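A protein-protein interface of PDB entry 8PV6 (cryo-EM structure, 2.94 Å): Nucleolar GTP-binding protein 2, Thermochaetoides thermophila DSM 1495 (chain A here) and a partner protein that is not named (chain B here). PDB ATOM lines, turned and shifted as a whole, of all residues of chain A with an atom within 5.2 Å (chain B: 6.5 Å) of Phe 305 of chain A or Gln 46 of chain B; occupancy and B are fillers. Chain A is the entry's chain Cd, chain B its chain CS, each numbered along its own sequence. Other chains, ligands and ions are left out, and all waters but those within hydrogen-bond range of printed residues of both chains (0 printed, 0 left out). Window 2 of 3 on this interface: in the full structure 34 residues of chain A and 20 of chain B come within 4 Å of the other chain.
The side-chain amide nitrogen of Gln 46 of chain B lies within hydrogen-bond range of the backbone carbonyl oxygen of Ala 296 of chain A (2.7 Å). OG of Ser 309 of chain A is in hydrogen-bond range of O of Asn 45 of chain B, 2.4 Å away.
The backbone carbonyl oxygen (O) of Arg 298 of chain A is in hydrogen-bond range of the backbone NH (N) of Phe 305 of chain A.
Leu 49 of chain B touches Ile 273 of chain A. Thr 294 of chain A touches Val 44 of chain B (O to CG1, 3.4 Å). Cys 295 of chain A touches Val 44 of chain B (SG to CG1, 3.7 Å). CA of Cys 295 of chain A touches OE1 of Gln 46 of chain B, at 3.5 Å. CE2 of Phe 305 of chain A touches NE2 of Gln 46 of chain B, at 3.5 Å. CA of Gly 306 of chain A touches NE2 of Gln 46 of chain B (3.7 Å). Ser 309 of chain A touches Gln 46 of chain B.
Of chain A, only Cys 295 (3.5 Å), Ala 296 (2.7 Å), Phe 305 (3.5 Å), Gly 306 (3.7 Å) and Ser 309 (3.5 Å) come within 4 Å of Gln 46 of chain B. Printed residues of chain B within 4 Å of Thr 294 of chain A: Val 44. Printed residues of chain A within 4 Å of Leu 49 of chain B: Ile 273 (3.8 Å). Printed residues of chain B within 4 Å of Gly 306 of chain A: Gln 46 (3.7 Å). Printed residues of chain B within 4 Å of Ala 296 of chain A: Gln 46 (2.7 Å). Thr 48 of chain B touches none of the printed residues of chain A. The nearest residue of chain A that does not touch Gln 46 of chain B is Thr 294 of chain A (4.3 Å). The nearest printed residue of chain A that does not touch Val 44 of chain B is Ser 309 of chain A (5.0 Å).
Hydrophobic or aromatic side chains of chain B that line the printed part of chain A: Val 44 and Leu 49. Hydrophobic or aromatic side chains of chain A that line the printed part of chain B: Ile 273, Ala 296 and Phe 305. Among the printed residues, 9 pairs touch across the chains. Among the printed residues, no Asp or Glu carboxylate lies within 4 Å of a Lys or Arg side-chain nitrogen of the other chain.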
ATOM      1  N   ILE A 273      -8.036   9.696 -14.739  1.00  0.00           N
ATOM      2  CA  ILE A 273      -7.582   8.750 -13.721  1.00  0.00           C
ATOM      3  C   ILE A 273      -7.852   7.305 -14.096  1.00  0.00           C
ATOM      4  O   ILE A 273      -7.379   6.399 -13.399  1.00  0.00           O
ATOM      5  CB  ILE A 273      -8.231   8.998 -12.346  1.00  0.00           C
ATOM      6  CG1 ILE A 273      -9.702   8.588 -12.370  1.00  0.00           C
ATOM      7  CG2 ILE A 273      -8.082  10.449 -11.942  1.00  0.00           C
ATOM      8  CD1 ILE A 273     -10.303   8.452 -11.005  1.00  0.00           C
ATOM      9  N   THR A 294      -7.879  19.163  -4.034  1.00  0.00           N
ATOM     10  CA  THR A 294      -7.730  18.316  -5.206  1.00  0.00           C
ATOM     11  C   THR A 294      -8.947  17.418  -5.367  1.00  0.00           C
ATOM     12  O   THR A 294      -9.433  16.820  -4.403  1.00  0.00           O
ATOM     13  CB  THR A 294      -6.460  17.454  -5.104  1.00  0.00           C
ATOM     14  OG1 THR A 294      -5.348  18.284  -4.751  1.00  0.00           O
ATOM     15  CG2 THR A 294      -6.161  16.764  -6.423  1.00  0.00           C
ATOM     16  N   CYS A 295      -9.437  17.331  -6.601  1.00  0.00           N
ATOM     17  CA  CYS A 295     -10.509  16.416  -6.957  1.00  0.00           C
ATOM     18  C   CYS A 295     -10.054  15.508  -8.090  1.00  0.00           C
ATOM     19  O   CYS A 295      -9.572  15.978  -9.121  1.00  0.00           O
ATOM     20  CB  CYS A 295     -11.777  17.162  -7.389  1.00  0.00           C
ATOM     21  SG  CYS A 295     -12.553  18.157  -6.103  1.00  0.00           S
ATOM     22  N   ALA A 296     -10.212  14.204  -7.896  1.00  0.00           N
ATOM     23  CA  ALA A 296      -9.994  13.231  -8.954  1.00  0.00           C
ATOM     24  C   ALA A 296     -11.245  13.136  -9.812  1.00  0.00           C
ATOM     25  O   ALA A 296     -12.368  13.211  -9.305  1.00  0.00           O
ATOM     26  CB  ALA A 296      -9.655  11.851  -8.391  1.00  0.00           C
ATOM     27  N   MET A 297     -11.054  12.969 -11.118  1.00  0.00           N
ATOM     28  CA  MET A 297     -12.205  13.008 -12.005  1.00  0.00           C
ATOM     29  C   MET A 297     -11.907  12.218 -13.270  1.00  0.00           C
ATOM     30  O   MET A 297     -10.803  12.274 -13.815  1.00  0.00           O
ATOM     31  CB  MET A 297     -12.588  14.458 -12.332  1.00  0.00           C
ATOM     32  CG  MET A 297     -13.725  14.619 -13.319  1.00  0.00           C
ATOM     33  SD  MET A 297     -14.606  16.169 -13.080  1.00  0.00           S
ATOM     34  CE  MET A 297     -16.123  15.818 -13.955  1.00  0.00           C
ATOM     35  N   ARG A 298     -12.906  11.461 -13.716  1.00  0.00           N
ATOM     36  CA  ARG A 298     -12.937  10.886 -15.057  1.00  0.00           C
ATOM     37  C   ARG A 298     -14.003  11.639 -15.839  1.00  0.00           C
ATOM     38  O   ARG A 298     -15.199  11.471 -15.585  1.00  0.00           O
ATOM     39  CB  ARG A 298     -13.231   9.388 -15.024  1.00  0.00           C
ATOM     40  CG  ARG A 298     -13.414   8.787 -16.405  1.00  0.00           C
ATOM     41  CD  ARG A 298     -13.652   7.292 -16.354  1.00  0.00           C
ATOM     42  NE  ARG A 298     -13.772   6.730 -17.694  1.00  0.00           N
ATOM     43  CZ  ARG A 298     -13.887   5.436 -17.959  1.00  0.00           C
ATOM     44  NH1 ARG A 298     -13.882   4.529 -16.996  1.00  0.00           N
ATOM     45  NH2 ARG A 298     -14.003   5.041 -19.223  1.00  0.00           N
ATOM     46  N   ASN A 303     -20.430   8.194 -18.292  1.00  0.00           N
ATOM     47  CA  ASN A 303     -19.934   7.561 -17.069  1.00  0.00           C
ATOM     48  C   ASN A 303     -18.852   8.427 -16.438  1.00  0.00           C
ATOM     49  O   ASN A 303     -17.654   8.164 -16.608  1.00  0.00           O
ATOM     50  CB  ASN A 303     -19.400   6.158 -17.357  1.00  0.00           C
ATOM     51  CG  ASN A 303     -20.503   5.164 -17.657  1.00  0.00           C
ATOM     52  OD1 ASN A 303     -21.683   5.448 -17.455  1.00  0.00           O
ATOM     53  ND2 ASN A 303     -20.123   3.988 -18.141  1.00  0.00           N
ATOM     54  N   PRO A 304     -19.235   9.462 -15.696  1.00  0.00           N
ATOM     55  CA  PRO A 304     -18.246  10.293 -15.010  1.00  0.00           C
ATOM     56  C   PRO A 304     -17.882   9.749 -13.635  1.00  0.00           C
ATOM     57  O   PRO A 304     -18.531   8.857 -13.089  1.00  0.00           O
ATOM     58  CB  PRO A 304     -18.966  11.640 -14.880  1.00  0.00           C
ATOM     59  CG  PRO A 304     -20.400  11.267 -14.752  1.00  0.00           C
ATOM     60  CD  PRO A 304     -20.604   9.974 -15.506  1.00  0.00           C
ATOM     61  N   PHE A 305     -16.813  10.315 -13.083  1.00  0.00           N
ATOM     62  CA  PHE A 305     -16.407  10.066 -11.707  1.00  0.00           C
ATOM     63  C   PHE A 305     -15.954  11.386 -11.102  1.00  0.00           C
ATOM     64  O   PHE A 305     -15.358  12.211 -11.798  1.00  0.00           O
ATOM     65  CB  PHE A 305     -15.288   9.025 -11.629  1.00  0.00           C
ATOM     66  CG  PHE A 305     -14.777   8.790 -10.237  1.00  0.00           C
ATOM     67  CD1 PHE A 305     -15.527   8.070  -9.322  1.00  0.00           C
ATOM     68  CD2 PHE A 305     -13.551   9.289  -9.840  1.00  0.00           C
ATOM     69  CE1 PHE A 305     -15.060   7.854  -8.041  1.00  0.00           C
ATOM     70  CE2 PHE A 305     -13.079   9.074  -8.562  1.00  0.00           C
ATOM     71  CZ  PHE A 305     -13.835   8.354  -7.663  1.00  0.00           C
ATOM     72  N   GLY A 306     -16.261  11.597  -9.826  1.00  0.00           N
ATOM     73  CA  GLY A 306     -15.882  12.818  -9.146  1.00  0.00           C
ATOM     74  C   GLY A 306     -16.749  14.014  -9.463  1.00  0.00           C
ATOM     75  O   GLY A 306     -16.469  15.114  -8.963  1.00  0.00           O
ATOM     76  N   ARG A 307     -17.791  13.829 -10.275  1.00  0.00           N
ATOM     77  CA  ARG A 307     -18.670  14.928 -10.653  1.00  0.00           C
ATOM     78  C   ARG A 307     -19.425  15.469  -9.448  1.00  0.00           C
ATOM     79  O   ARG A 307     -19.549  16.687  -9.276  1.00  0.00           O
ATOM     80  CB  ARG A 307     -19.637  14.452 -11.738  1.00  0.00           C
ATOM     81  CG  ARG A 307     -20.638  15.484 -12.204  1.00  0.00           C
ATOM     82  CD  ARG A 307     -21.684  14.834 -13.087  1.00  0.00           C
ATOM     83  NE  ARG A 307     -22.588  15.809 -13.680  1.00  0.00           N
ATOM     84  CZ  ARG A 307     -23.689  16.260 -13.097  1.00  0.00           C
ATOM     85  NH1 ARG A 307     -24.064  15.828 -11.905  1.00  0.00           N
ATOM     86  NH2 ARG A 307     -24.433  17.164 -13.726  1.00  0.00           N
ATOM     87  N   SER A 309     -18.511  15.276  -6.266  1.00  0.00           N
ATOM     88  CA  SER A 309     -17.557  15.955  -5.396  1.00  0.00           C
ATOM     89  C   SER A 309     -17.196  17.334  -5.931  1.00  0.00           C
ATOM     90  O   SER A 309     -17.094  18.301  -5.163  1.00  0.00           O
ATOM     91  CB  SER A 309     -16.302  15.101  -5.235  1.00  0.00           C
ATOM     92  OG  SER A 309     -16.600  13.884  -4.581  1.00  0.00           O
ATOM     93  N   VAL B  44     -12.964  18.738   0.652  1.00  0.00           N
ATOM     94  CA  VAL B  44     -13.285  17.992  -0.557  1.00  0.00           C
ATOM     95  C   VAL B  44     -13.943  16.684  -0.144  1.00  0.00           C
ATOM     96  O   VAL B  44     -13.339  15.871   0.566  1.00  0.00           O
ATOM     97  CB  VAL B  44     -12.034  17.735  -1.410  1.00  0.00           C
ATOM     98  CG1 VAL B  44     -12.398  16.950  -2.653  1.00  0.00           C
ATOM     99  CG2 VAL B  44     -11.371  19.048  -1.784  1.00  0.00           C
ATOM    100  N   ASN B  45     -15.180  16.478  -0.589  1.00  0.00           N
ATOM    101  CA  ASN B  45     -15.967  15.302  -0.224  1.00  0.00           C
ATOM    102  C   ASN B  45     -15.733  14.226  -1.277  1.00  0.00           C
ATOM    103  O   ASN B  45     -16.580  13.974  -2.133  1.00  0.00           O
ATOM    104  CB  ASN B  45     -17.442  15.661  -0.109  1.00  0.00           C
ATOM    105  CG  ASN B  45     -17.689  16.800   0.852  1.00  0.00           C
ATOM    106  OD1 ASN B  45     -16.767  17.289   1.504  1.00  0.00           O
ATOM    107  ND2 ASN B  45     -18.935  17.246   0.931  1.00  0.00           N
ATOM    108  N   GLN B  46     -14.570  13.584  -1.210  1.00  0.00           N
ATOM    109  CA  GLN B  46     -14.249  12.504  -2.132  1.00  0.00           C
ATOM    110  C   GLN B  46     -13.475  11.436  -1.377  1.00  0.00           C
ATOM    111  O   GLN B  46     -12.491  11.745  -0.699  1.00  0.00           O
ATOM    112  CB  GLN B  46     -13.440  13.015  -3.328  1.00  0.00           C
ATOM    113  CG  GLN B  46     -13.407  12.053  -4.501  1.00  0.00           C
ATOM    114  CD  GLN B  46     -12.701  12.629  -5.707  1.00  0.00           C
ATOM    115  OE1 GLN B  46     -11.902  13.555  -5.586  1.00  0.00           O
ATOM    116  NE2 GLN B  46     -12.994  12.086  -6.880  1.00  0.00           N
ATOM    117  N   GLN B  47     -13.921  10.190  -1.498  1.00  0.00           N
ATOM    118  CA  GLN B  47     -13.302   9.092  -0.775  1.00  0.00           C
ATOM    119  C   GLN B  47     -11.953   8.725  -1.387  1.00  0.00           C
ATOM    120  O   GLN B  47     -11.591   9.169  -2.481  1.00  0.00           O
ATOM    121  CB  GLN B  47     -14.219   7.869  -0.772  1.00  0.00           C
ATOM    122  CG  GLN B  47     -15.605   8.132  -0.214  1.00  0.00           C
ATOM    123  CD  GLN B  47     -16.525   6.936  -0.356  1.00  0.00           C
ATOM    124  OE1 GLN B  47     -16.117   5.880  -0.840  1.00  0.00           O
ATOM    125  NE2 GLN B  47     -17.775   7.096   0.064  1.00  0.00           N
ATOM    126  N   THR B  48     -11.204   7.909  -0.649  1.00  0.00           N
ATOM    127  CA  THR B  48      -9.936   7.388  -1.135  1.00  0.00           C
ATOM    128  C   THR B  48     -10.173   6.466  -2.330  1.00  0.00           C
ATOM    129  O   THR B  48     -11.092   5.645  -2.343  1.00  0.00           O
ATOM    130  CB  THR B  48      -9.211   6.645  -0.009  1.00  0.00           C
ATOM    131  OG1 THR B  48      -9.014   7.532   1.097  1.00  0.00           O
ATOM    132  CG2 THR B  48      -7.852   6.132  -0.468  1.00  0.00           C
ATOM    133  N   LEU B  49      -9.340   6.628  -3.358  1.00  0.00           N
ATOM    134  CA  LEU B  49      -9.512   5.891  -4.604  1.00  0.00           C
ATOM    135  C   LEU B  49      -9.112   4.424  -4.492  1.00  0.00           C
ATOM    136  O   LEU B  49      -9.778   3.560  -5.071  1.00  0.00           O
ATOM    137  CB  LEU B  49      -8.711   6.560  -5.724  1.00  0.00           C
ATOM    138  CG  LEU B  49      -9.451   7.526  -6.654  1.00  0.00           C
ATOM    139  CD1 LEU B  49     -10.081   8.685  -5.897  1.00  0.00           C
ATOM    140  CD2 LEU B  49      -8.506   8.043  -7.719  1.00  0.00           C
